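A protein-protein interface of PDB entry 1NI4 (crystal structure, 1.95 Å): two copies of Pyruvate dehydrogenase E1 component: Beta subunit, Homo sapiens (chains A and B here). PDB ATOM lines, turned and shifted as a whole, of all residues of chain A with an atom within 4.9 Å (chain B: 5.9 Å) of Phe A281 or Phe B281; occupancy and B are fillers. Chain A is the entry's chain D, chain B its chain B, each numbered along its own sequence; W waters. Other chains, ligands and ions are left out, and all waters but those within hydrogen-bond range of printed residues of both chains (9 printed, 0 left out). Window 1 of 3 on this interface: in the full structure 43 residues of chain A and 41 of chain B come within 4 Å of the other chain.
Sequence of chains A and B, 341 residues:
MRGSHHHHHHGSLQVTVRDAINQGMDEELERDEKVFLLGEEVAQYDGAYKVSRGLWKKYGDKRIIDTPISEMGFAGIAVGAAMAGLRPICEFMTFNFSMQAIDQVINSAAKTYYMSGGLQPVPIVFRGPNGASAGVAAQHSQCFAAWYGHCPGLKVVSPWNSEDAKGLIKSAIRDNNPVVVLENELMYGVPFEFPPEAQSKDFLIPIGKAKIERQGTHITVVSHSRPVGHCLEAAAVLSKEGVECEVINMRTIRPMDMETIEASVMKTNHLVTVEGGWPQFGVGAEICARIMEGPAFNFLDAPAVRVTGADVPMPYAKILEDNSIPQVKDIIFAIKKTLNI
Among the printed residues, pairs that only touch across the chains: Ala A146 with Phe B281, Gly A149 with Phe B281, His A150 with Trp B278, His A150 with Phe B281, Ile A253 with Phe B281, Met A256 with Phe B281, Gln A280 with Glu B286, Phe A281 with Ala B146, Phe A281 with Gly B149, Phe A281 with His B150, Phe A281 with Ile B253, Phe A281 with Met B256, Phe A281 with Phe B281, Phe A281 with Gly B282, Phe A281 with Val B283, Gly A282 with Phe B281, Val A283 with Phe B281, Ala A285 with Ala B285, Ala A285 with Glu B286, Glu A286 with Gln B280 and Glu A286 with Ala B285.
Hydrophobic or aromatic side chains of chain A within 4 Å of the printed part of chain B: His A150, Ile A253, Met A256, Phe A281, Val A283 and Ala A285.
Phe A281 touches just these residues of chain B: Ala B146, Gly B149, His B150, Ile B253, Met B256, Phe B281, Gly B282, Val B283 and Glu B286.
Of the printed residues of chain A, Phe B281 touches Ala A146 (3.8 Å), Gly A149 (3.3 Å), His A150 (3.7 Å), Ile A253 (3.8 Å), Met A256 (3.3 Å), Phe A281 (3.9 Å), Gly A282 (3.6 Å), Val A283 (3.5 Å) and Glu A286 (2.7 Å).
Of the printed residues of chain B, Ala A146 touches Phe B281 (3.8 Å).
Of the printed residues of chain A, Trp B278 touches His A150.
Printed residues of chain B within 4 Å of Ala A285: Ala B285 and Glu B286.
The nearest printed residue of chain A that does not touch Phe B281 is Ala A285 (6.0 Å).
Water W8 lies within hydrogen-bond range of OE1 of Gln A280 (2.6 Å), O of Ile B253 (2.7 Å) and N of Met B256 (2.8 Å).
Water W1 bridges NE2 of His A150 (2.7 Å) and N of Trp B278 (3.2 Å).
Water W4 bridges the backbone carbonyl oxygen of His A150 (3.0 Å) and the backbone NH of Gln B280 (3.2 Å).
Water W6 lies within hydrogen-bond range of N of Ala A146 (3.1 Å) and NE2 of His B150 (3.3 Å).
Water W3 lies within hydrogen-bond range of N of Ala B146 and NE2 of His A150.
Water W7 bridges the backbone carbonyl oxygen of Ala A146 (3.2 Å) and the backbone carbonyl oxygen of Phe B281 (3.3 Å).
The backbone carbonyl oxygen of Gln A280 lies within hydrogen-bond range of a ring nitrogen (ND1) of His B150.
The guanidinium group of Arg B254 lies close to the side-chain amide nitrogen of Gln A280 (3.2 Å).
O of Gln B280 is in hydrogen-bond range of ND1 of His A150 (2.7 Å).
OE1 of Glu A286 sits at hydrogen-bond distance from N of Phe B281, 2.7 Å away.
OE1 of Glu B286 sits at hydrogen-bond distance from N of Phe A281 (2.8 Å).
The guanidinium group (NH1) of Arg B306 lies within salt-bridge range of the side-chain carboxylate (OE1) of Glu A286, 3.2 Å away.
The backbone carbonyl oxygen (O) of Pro A279 sits close to the side-chain carboxylate (OE1) of Glu B286, 3.4 Å away.
The side-chain carboxylate (OE1) of Glu A286 sits close to the backbone carbonyl oxygen (O) of Pro B279, at 3.5 Å.
The backbone carbonyl oxygen of Gly B149 lies within hydrogen-bond range of the guanidinium group of Arg B254.
The backbone carbonyl oxygen (O) of Pro B279 lies within hydrogen-bond range of the guanidinium group (NH1) of Arg B306 (2.9 Å).
Ala A146 touches Phe B281, and with the chains exchanged Phe A281 touches Ala B146.
His A150 touches Phe B281, and with the chains exchanged Phe A281 touches His B150.
Met A256 touches Phe B281, and with the chains exchanged Phe A281 touches Met B256.
Phe A281 touches Val B283, and with the chains exchanged Val A283 touches Phe B281.
Positions printed for both chains: 146, 149, 150, 253, 256, 279, 280, 281, 282, 283, 285 and 286.
Of the 29 pairs that touch across the chains among the printed residues, 26 have their exchanged pair printed and touching as well.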
ATOM      1  N   ALA A 146     -29.183  15.339  -0.925  1.00  0.00           N
ATOM      2  CA  ALA A 146     -28.079  15.701  -0.038  1.00  0.00           C
ATOM      3  C   ALA A 146     -28.479  15.900   1.424  1.00  0.00           C
ATOM      4  O   ALA A 146     -27.741  15.517   2.324  1.00  0.00           O
ATOM      5  CB  ALA A 146     -27.386  16.954  -0.565  1.00  0.00           C
ATOM      6  N   GLY A 149     -29.360  12.340   2.746  1.00  0.00           N
ATOM      7  CA  GLY A 149     -28.180  11.496   2.665  1.00  0.00           C
ATOM      8  C   GLY A 149     -27.121  11.845   3.694  1.00  0.00           C
ATOM      9  O   GLY A 149     -26.162  11.105   3.891  1.00  0.00           O
ATOM     10  N   HIS A 150     -27.322  12.978   4.358  1.00  0.00           N
ATOM     11  CA  HIS A 150     -26.410  13.506   5.368  1.00  0.00           C
ATOM     12  C   HIS A 150     -26.603  12.874   6.753  1.00  0.00           C
ATOM     13  O   HIS A 150     -25.694  12.903   7.587  1.00  0.00           O
ATOM     14  CB  HIS A 150     -26.634  15.027   5.443  1.00  0.00           C
ATOM     15  CG  HIS A 150     -25.765  15.744   6.432  1.00  0.00           C
ATOM     16  ND1 HIS A 150     -24.412  15.934   6.244  1.00  0.00           N
ATOM     17  CD2 HIS A 150     -26.073  16.373   7.593  1.00  0.00           C
ATOM     18  CE1 HIS A 150     -23.925  16.651   7.240  1.00  0.00           C
ATOM     19  NE2 HIS A 150     -24.913  16.931   8.073  1.00  0.00           N
ATOM     20  N   ILE A 253     -28.156   6.811  -2.464  1.00  0.00           N
ATOM     21  CA  ILE A 253     -27.482   8.037  -2.052  1.00  0.00           C
ATOM     22  C   ILE A 253     -26.739   7.758  -0.751  1.00  0.00           C
ATOM     23  O   ILE A 253     -25.639   8.263  -0.528  1.00  0.00           O
ATOM     24  CB  ILE A 253     -28.495   9.189  -1.819  1.00  0.00           C
ATOM     25  CG1 ILE A 253     -29.368   9.378  -3.063  1.00  0.00           C
ATOM     26  CG2 ILE A 253     -27.758  10.477  -1.485  1.00  0.00           C
ATOM     27  CD1 ILE A 253     -28.581   9.633  -4.341  1.00  0.00           C
ATOM     28  N   MET A 256     -23.815   5.207  -0.319  1.00  0.00           N
ATOM     29  CA  MET A 256     -23.432   5.137  -1.727  1.00  0.00           C
ATOM     30  C   MET A 256     -22.321   4.131  -2.017  1.00  0.00           C
ATOM     31  O   MET A 256     -21.458   3.872  -1.178  1.00  0.00           O
ATOM     32  CB  MET A 256     -23.031   6.523  -2.254  1.00  0.00           C
ATOM     33  CG  MET A 256     -21.892   7.201  -1.512  1.00  0.00           C
ATOM     34  SD  MET A 256     -21.319   8.817  -2.427  1.00  0.00           S
ATOM     35  CE  MET A 256     -22.645  10.049  -1.757  1.00  0.00           C
ATOM     36  N   PRO A 279     -25.760  22.956  -6.231  1.00  0.00           N
ATOM     37  CA  PRO A 279     -24.348  22.559  -6.128  1.00  0.00           C
ATOM     38  C   PRO A 279     -23.655  22.559  -4.760  1.00  0.00           C
ATOM     39  O   PRO A 279     -22.954  21.604  -4.420  1.00  0.00           O
ATOM     40  CB  PRO A 279     -23.660  23.496  -7.119  1.00  0.00           C
ATOM     41  CG  PRO A 279     -24.478  24.745  -7.002  1.00  0.00           C
ATOM     42  CD  PRO A 279     -25.896  24.213  -6.989  1.00  0.00           C
ATOM     43  N   GLN A 280     -23.847  23.605  -3.970  1.00  0.00           N
ATOM     44  CA  GLN A 280     -23.170  23.676  -2.683  1.00  0.00           C
ATOM     45  C   GLN A 280     -23.632  22.655  -1.650  1.00  0.00           C
ATOM     46  O   GLN A 280     -24.788  22.644  -1.235  1.00  0.00           O
ATOM     47  CB  GLN A 280     -23.277  25.093  -2.124  1.00  0.00           C
ATOM     48  CG  GLN A 280     -22.731  26.140  -3.083  1.00  0.00           C
ATOM     49  CD  GLN A 280     -22.557  27.498  -2.433  1.00  0.00           C
ATOM     50  OE1 GLN A 280     -21.827  27.637  -1.451  1.00  0.00           O
ATOM     51  NE2 GLN A 280     -23.222  28.509  -2.980  1.00  0.00           N
ATOM     52  N   PHE A 281     -22.703  21.803  -1.226  1.00  0.00           N
ATOM     53  CA  PHE A 281     -22.998  20.766  -0.247  1.00  0.00           C
ATOM     54  C   PHE A 281     -23.932  19.726  -0.866  1.00  0.00           C
ATOM     55  O   PHE A 281     -24.674  19.050  -0.166  1.00  0.00           O
ATOM     56  CB  PHE A 281     -23.641  21.386   1.002  1.00  0.00           C
ATOM     57  CG  PHE A 281     -22.879  22.562   1.550  1.00  0.00           C
ATOM     58  CD1 PHE A 281     -21.668  22.382   2.200  1.00  0.00           C
ATOM     59  CD2 PHE A 281     -23.355  23.858   1.375  1.00  0.00           C
ATOM     60  CE1 PHE A 281     -20.937  23.477   2.668  1.00  0.00           C
ATOM     61  CE2 PHE A 281     -22.634  24.958   1.836  1.00  0.00           C
ATOM     62  CZ  PHE A 281     -21.426  24.770   2.481  1.00  0.00           C
ATOM     63  N   GLY A 282     -23.880  19.602  -2.186  1.00  0.00           N
ATOM     64  CA  GLY A 282     -24.728  18.645  -2.869  1.00  0.00           C
ATOM     65  C   GLY A 282     -24.092  17.281  -3.039  1.00  0.00           C
ATOM     66  O   GLY A 282     -23.007  17.011  -2.522  1.00  0.00           O
ATOM     67  N   VAL A 283     -24.775  16.419  -3.781  1.00  0.00           N
ATOM     68  CA  VAL A 283     -24.306  15.062  -4.029  1.00  0.00           C
ATOM     69  C   VAL A 283     -22.975  14.995  -4.768  1.00  0.00           C
ATOM     70  O   VAL A 283     -22.142  14.133  -4.486  1.00  0.00           O
ATOM     71  CB  VAL A 283     -25.365  14.262  -4.817  1.00  0.00           C
ATOM     72  CG1 VAL A 283     -24.812  12.902  -5.204  1.00  0.00           C
ATOM     73  CG2 VAL A 283     -26.629  14.109  -3.965  1.00  0.00           C
ATOM     74  N   ALA A 285     -20.511  17.102  -4.621  1.00  0.00           N
ATOM     75  CA  ALA A 285     -19.414  17.480  -3.741  1.00  0.00           C
ATOM     76  C   ALA A 285     -18.906  16.280  -2.952  1.00  0.00           C
ATOM     77  O   ALA A 285     -17.696  16.089  -2.802  1.00  0.00           O
ATOM     78  CB  ALA A 285     -19.865  18.586  -2.782  1.00  0.00           C
ATOM     79  N   GLU A 286     -19.836  15.472  -2.447  1.00  0.00           N
ATOM     80  CA  GLU A 286     -19.474  14.299  -1.661  1.00  0.00           C
ATOM     81  C   GLU A 286     -18.696  13.282  -2.493  1.00  0.00           C
ATOM     82  O   GLU A 286     -17.717  12.703  -2.019  1.00  0.00           O
ATOM     83  CB  GLU A 286     -20.730  13.659  -1.065  1.00  0.00           C
ATOM     84  CG  GLU A 286     -20.463  12.494  -0.114  1.00  0.00           C
ATOM     85  CD  GLU A 286     -19.458  12.830   0.983  1.00  0.00           C
ATOM     86  OE1 GLU A 286     -19.418  13.994   1.439  1.00  0.00           O
ATOM     87  OE2 GLU A 286     -18.712  11.920   1.403  1.00  0.00           O
ATOM     88  N   ALA B 145     -24.897  23.310   9.802  1.00  0.00           N
ATOM     89  CA  ALA B 145     -24.165  24.176   8.880  1.00  0.00           C
ATOM     90  C   ALA B 145     -24.363  23.752   7.423  1.00  0.00           C
ATOM     91  O   ALA B 145     -24.682  24.578   6.563  1.00  0.00           O
ATOM     92  CB  ALA B 145     -22.679  24.169   9.222  1.00  0.00           C
ATOM     93  N   ALA B 146     -24.186  22.462   7.156  1.00  0.00           N
ATOM     94  CA  ALA B 146     -24.329  21.936   5.805  1.00  0.00           C
ATOM     95  C   ALA B 146     -25.750  22.071   5.265  1.00  0.00           C
ATOM     96  O   ALA B 146     -25.947  22.361   4.083  1.00  0.00           O
ATOM     97  CB  ALA B 146     -23.893  20.478   5.769  1.00  0.00           C
ATOM     98  N   GLY B 149     -26.483  26.032   4.672  1.00  0.00           N
ATOM     99  CA  GLY B 149     -25.557  26.584   3.697  1.00  0.00           C
ATOM    100  C   GLY B 149     -25.807  26.088   2.286  1.00  0.00           C
ATOM    101  O   GLY B 149     -25.232  26.591   1.326  1.00  0.00           O
ATOM    102  N   HIS B 150     -26.681  25.098   2.171  1.00  0.00           N
ATOM    103  CA  HIS B 150     -27.040  24.491   0.898  1.00  0.00           C
ATOM    104  C   HIS B 150     -28.113  25.308   0.166  1.00  0.00           C
ATOM    105  O   HIS B 150     -28.254  25.188  -1.049  1.00  0.00           O
ATOM    106  CB  HIS B 150     -27.557  23.062   1.173  1.00  0.00           C
ATOM    107  CG  HIS B 150     -28.012  22.309  -0.044  1.00  0.00           C
ATOM    108  ND1 HIS B 150     -27.148  21.882  -1.029  1.00  0.00           N
ATOM    109  CD2 HIS B 150     -29.236  21.852  -0.400  1.00  0.00           C
ATOM    110  CE1 HIS B 150     -27.816  21.194  -1.937  1.00  0.00           C
ATOM    111  NE2 HIS B 150     -29.087  21.161  -1.579  1.00  0.00           N
ATOM    112  N   ILE B 253     -20.476  30.442   6.141  1.00  0.00           N
ATOM    113  CA  ILE B 253     -20.693  29.158   5.482  1.00  0.00           C
ATOM    114  C   ILE B 253     -21.234  29.434   4.080  1.00  0.00           C
ATOM    115  O   ILE B 253     -20.850  28.782   3.112  1.00  0.00           O
ATOM    116  CB  ILE B 253     -21.710  28.290   6.264  1.00  0.00           C
ATOM    117  CG1 ILE B 253     -21.197  28.053   7.684  1.00  0.00           C
ATOM    118  CG2 ILE B 253     -21.943  26.963   5.543  1.00  0.00           C
ATOM    119  CD1 ILE B 253     -19.810  27.405   7.753  1.00  0.00           C
ATOM    120  N   ARG B 254     -22.132  30.408   3.982  1.00  0.00           N
ATOM    121  CA  ARG B 254     -22.716  30.791   2.701  1.00  0.00           C
ATOM    122  C   ARG B 254     -22.981  32.298   2.692  1.00  0.00           C
ATOM    123  O   ARG B 254     -23.753  32.803   3.506  1.00  0.00           O
ATOM    124  CB  ARG B 254     -24.034  30.051   2.463  1.00  0.00           C
ATOM    125  CG  ARG B 254     -24.532  30.174   1.025  1.00  0.00           C
ATOM    126  CD  ARG B 254     -26.015  29.849   0.862  1.00  0.00           C
ATOM    127  NE  ARG B 254     -26.428  30.070  -0.522  1.00  0.00           N
ATOM    128  CZ  ARG B 254     -26.315  29.168  -1.490  1.00  0.00           C
ATOM    129  NH1 ARG B 254     -25.815  27.966  -1.231  1.00  0.00           N
ATOM    130  NH2 ARG B 254     -26.668  29.477  -2.725  1.00  0.00           N
ATOM    131  N   MET B 256     -19.346  31.319   1.339  1.00  0.00           N
ATOM    132  CA  MET B 256     -18.014  31.146   1.905  1.00  0.00           C
ATOM    133  C   MET B 256     -16.936  31.875   1.111  1.00  0.00           C
ATOM    134  O   MET B 256     -17.085  32.122  -0.084  1.00  0.00           O
ATOM    135  CB  MET B 256     -17.660  29.659   2.015  1.00  0.00           C
ATOM    136  CG  MET B 256     -17.621  28.922   0.696  1.00  0.00           C
ATOM    137  SD  MET B 256     -16.986  27.112   0.937  1.00  0.00           S
ATOM    138  CE  MET B 256     -18.556  26.372   1.798  1.00  0.00           C
ATOM    139  N   TRP B 278     -21.401  15.836  10.705  1.00  0.00           N
ATOM    140  CA  TRP B 278     -21.266  14.553  10.012  1.00  0.00           C
ATOM    141  C   TRP B 278     -20.514  14.757   8.694  1.00  0.00           C
ATOM    142  O   TRP B 278     -20.700  15.765   8.015  1.00  0.00           O
ATOM    143  CB  TRP B 278     -22.650  13.927   9.752  1.00  0.00           C
ATOM    144  CG  TRP B 278     -23.381  13.566  11.013  1.00  0.00           C
ATOM    145  CD1 TRP B 278     -22.845  12.988  12.134  1.00  0.00           C
ATOM    146  CD2 TRP B 278     -24.772  13.770  11.294  1.00  0.00           C
ATOM    147  NE1 TRP B 278     -23.813  12.827  13.093  1.00  0.00           N
ATOM    148  CE2 TRP B 278     -25.005  13.297  12.606  1.00  0.00           C
ATOM    149  CE3 TRP B 278     -25.844  14.305  10.564  1.00  0.00           C
ATOM    150  CZ2 TRP B 278     -26.268  13.343  13.208  1.00  0.00           C
ATOM    151  CZ3 TRP B 278     -27.104  14.350  11.161  1.00  0.00           C
ATOM    152  CH2 TRP B 278     -27.303  13.871  12.472  1.00  0.00           C
ATOM    153  N   PRO B 279     -19.660  13.793   8.318  1.00  0.00           N
ATOM    154  CA  PRO B 279     -18.834  13.799   7.104  1.00  0.00           C
ATOM    155  C   PRO B 279     -19.493  13.840   5.723  1.00  0.00           C
ATOM    156  O   PRO B 279     -19.080  14.620   4.861  1.00  0.00           O
ATOM    157  CB  PRO B 279     -17.980  12.549   7.277  1.00  0.00           C
ATOM    158  CG  PRO B 279     -18.920  11.616   7.956  1.00  0.00           C
ATOM    159  CD  PRO B 279     -19.513  12.507   9.026  1.00  0.00           C
ATOM    160  N   GLN B 280     -20.510  13.017   5.496  1.00  0.00           N
ATOM    161  CA  GLN B 280     -21.128  12.977   4.177  1.00  0.00           C
ATOM    162  C   GLN B 280     -21.997  14.174   3.830  1.00  0.00           C
ATOM    163  O   GLN B 280     -22.936  14.505   4.546  1.00  0.00           O
ATOM    164  CB  GLN B 280     -21.908  11.676   4.021  1.00  0.00           C
ATOM    165  CG  GLN B 280     -21.063  10.462   4.374  1.00  0.00           C
ATOM    166  CD  GLN B 280     -21.728   9.161   3.999  1.00  0.00           C
ATOM    167  OE1 GLN B 280     -21.947   8.881   2.816  1.00  0.00           O
ATOM    168  NE2 GLN B 280     -22.056   8.355   5.002  1.00  0.00           N
ATOM    169  N   PHE B 281     -21.666  14.816   2.714  1.00  0.00           N
ATOM    170  CA  PHE B 281     -22.383  15.993   2.239  1.00  0.00           C
ATOM    171  C   PHE B 281     -22.155  17.167   3.178  1.00  0.00           C
ATOM    172  O   PHE B 281     -22.915  18.131   3.160  1.00  0.00           O
ATOM    173  CB  PHE B 281     -23.884  15.696   2.124  1.00  0.00           C
ATOM    174  CG  PHE B 281     -24.193  14.513   1.260  1.00  0.00           C
ATOM    175  CD1 PHE B 281     -23.954  14.555  -0.109  1.00  0.00           C
ATOM    176  CD2 PHE B 281     -24.661  13.334   1.822  1.00  0.00           C
ATOM    177  CE1 PHE B 281     -24.172  13.434  -0.906  1.00  0.00           C
ATOM    178  CE2 PHE B 281     -24.882  12.203   1.031  1.00  0.00           C
ATOM    179  CZ  PHE B 281     -24.635  12.255  -0.336  1.00  0.00           C
ATOM    180  N   GLY B 282     -21.097  17.083   3.982  1.00  0.00           N
ATOM    181  CA  GLY B 282     -20.781  18.142   4.931  1.00  0.00           C
ATOM    182  C   GLY B 282     -20.041  19.336   4.350  1.00  0.00           C
ATOM    183  O   GLY B 282     -19.856  19.438   3.133  1.00  0.00           O
ATOM    184  N   VAL B 283     -19.616  20.242   5.229  1.00  0.00           N
ATOM    185  CA  VAL B 283     -18.893  21.448   4.823  1.00  0.00           C
ATOM    186  C   VAL B 283     -17.565  21.109   4.153  1.00  0.00           C
ATOM    187  O   VAL B 283     -17.216  21.680   3.114  1.00  0.00           O
ATOM    188  CB  VAL B 283     -18.626  22.367   6.035  1.00  0.00           C
ATOM    189  CG1 VAL B 283     -17.901  23.631   5.590  1.00  0.00           C
ATOM    190  CG2 VAL B 283     -19.946  22.724   6.712  1.00  0.00           C
ATOM    191  N   GLY B 284     -16.831  20.173   4.750  1.00  0.00           N
ATOM    192  CA  GLY B 284     -15.554  19.770   4.195  1.00  0.00           C
ATOM    193  C   GLY B 284     -15.653  19.263   2.766  1.00  0.00           C
ATOM    194  O   GLY B 284     -14.740  19.471   1.965  1.00  0.00           O
ATOM    195  N   ALA B 285     -16.754  18.597   2.434  1.00  0.00           N
ATOM    196  CA  ALA B 285     -16.928  18.067   1.085  1.00  0.00           C
ATOM    197  C   ALA B 285     -16.992  19.191   0.059  1.00  0.00           C
ATOM    198  O   ALA B 285     -16.381  19.105  -1.001  1.00  0.00           O
ATOM    199  CB  ALA B 285     -18.191  17.211   1.006  1.00  0.00           C
ATOM    200  N   GLU B 286     -17.729  20.245   0.381  1.00  0.00           N
ATOM    201  CA  GLU B 286     -17.867  21.373  -0.526  1.00  0.00           C
ATOM    202  C   GLU B 286     -16.532  22.068  -0.741  1.00  0.00           C
ATOM    203  O   GLU B 286     -16.209  22.463  -1.858  1.00  0.00           O
ATOM    204  CB  GLU B 286     -18.889  22.374   0.014  1.00  0.00           C
ATOM    205  CG  GLU B 286     -19.147  23.561  -0.914  1.00  0.00           C
ATOM    206  CD  GLU B 286     -19.536  23.127  -2.319  1.00  0.00           C
ATOM    207  OE1 GLU B 286     -20.154  22.048  -2.455  1.00  0.00           O
ATOM    208  OE2 GLU B 286     -19.236  23.868  -3.283  1.00  0.00           O
ATOM    209  N   ILE B 287     -15.757  22.216   0.328  1.00  0.00           N
ATOM    210  CA  ILE B 287     -14.458  22.865   0.224  1.00  0.00           C
ATOM    211  C   ILE B 287     -13.523  22.058  -0.680  1.00  0.00           C
ATOM    212  O   ILE B 287     -12.835  22.626  -1.532  1.00  0.00           O
ATOM    213  CB  ILE B 287     -13.811  23.050   1.618  1.00  0.00           C
ATOM    214  CG1 ILE B 287     -14.650  24.029   2.444  1.00  0.00           C
ATOM    215  CG2 ILE B 287     -12.383  23.568   1.477  1.00  0.00           C
ATOM    216  CD1 ILE B 287     -14.138  24.255   3.844  1.00  0.00           C
ATOM    217  N   ARG B 306     -10.284  15.386   5.212  1.00  0.00           N
ATOM    218  CA  ARG B 306     -11.319  15.956   6.065  1.00  0.00           C
ATOM    219  C   ARG B 306     -11.332  15.369   7.466  1.00  0.00           C
ATOM    220  O   ARG B 306     -11.226  14.155   7.645  1.00  0.00           O
ATOM    221  CB  ARG B 306     -12.700  15.741   5.442  1.00  0.00           C
ATOM    222  CG  ARG B 306     -12.932  16.457   4.125  1.00  0.00           C
ATOM    223  CD  ARG B 306     -14.320  16.139   3.596  1.00  0.00           C
ATOM    224  NE  ARG B 306     -14.471  14.718   3.296  1.00  0.00           N
ATOM    225  CZ  ARG B 306     -15.640  14.119   3.072  1.00  0.00           C
ATOM    226  NH1 ARG B 306     -16.766  14.819   3.121  1.00  0.00           N
ATOM    227  NH2 ARG B 306     -15.682  12.822   2.784  1.00  0.00           N
HETATM  228  O   HOH W   1     -24.185  17.494  10.643  1.00  0.00           O
HETATM  229  O   HOH W   2     -23.628   7.070   1.927  1.00  0.00           O
HETATM  230  O   HOH W   3     -25.905  19.978   8.094  1.00  0.00           O
HETATM  231  O   HOH W   4     -22.906  11.758   7.131  1.00  0.00           O
HETATM  232  O   HOH W   5     -26.089  25.577  -3.364  1.00  0.00           O
HETATM  233  O   HOH W   6     -30.351  18.231  -0.754  1.00  0.00           O
HETATM  234  O   HOH W   7     -26.161  17.937   3.685  1.00  0.00           O
HETATM  235  O   HOH W   8     -20.757  29.048   0.406  1.00  0.00           O
HETATM  236  O   HOH W   9     -26.655  20.188   2.209  1.00  0.00           O
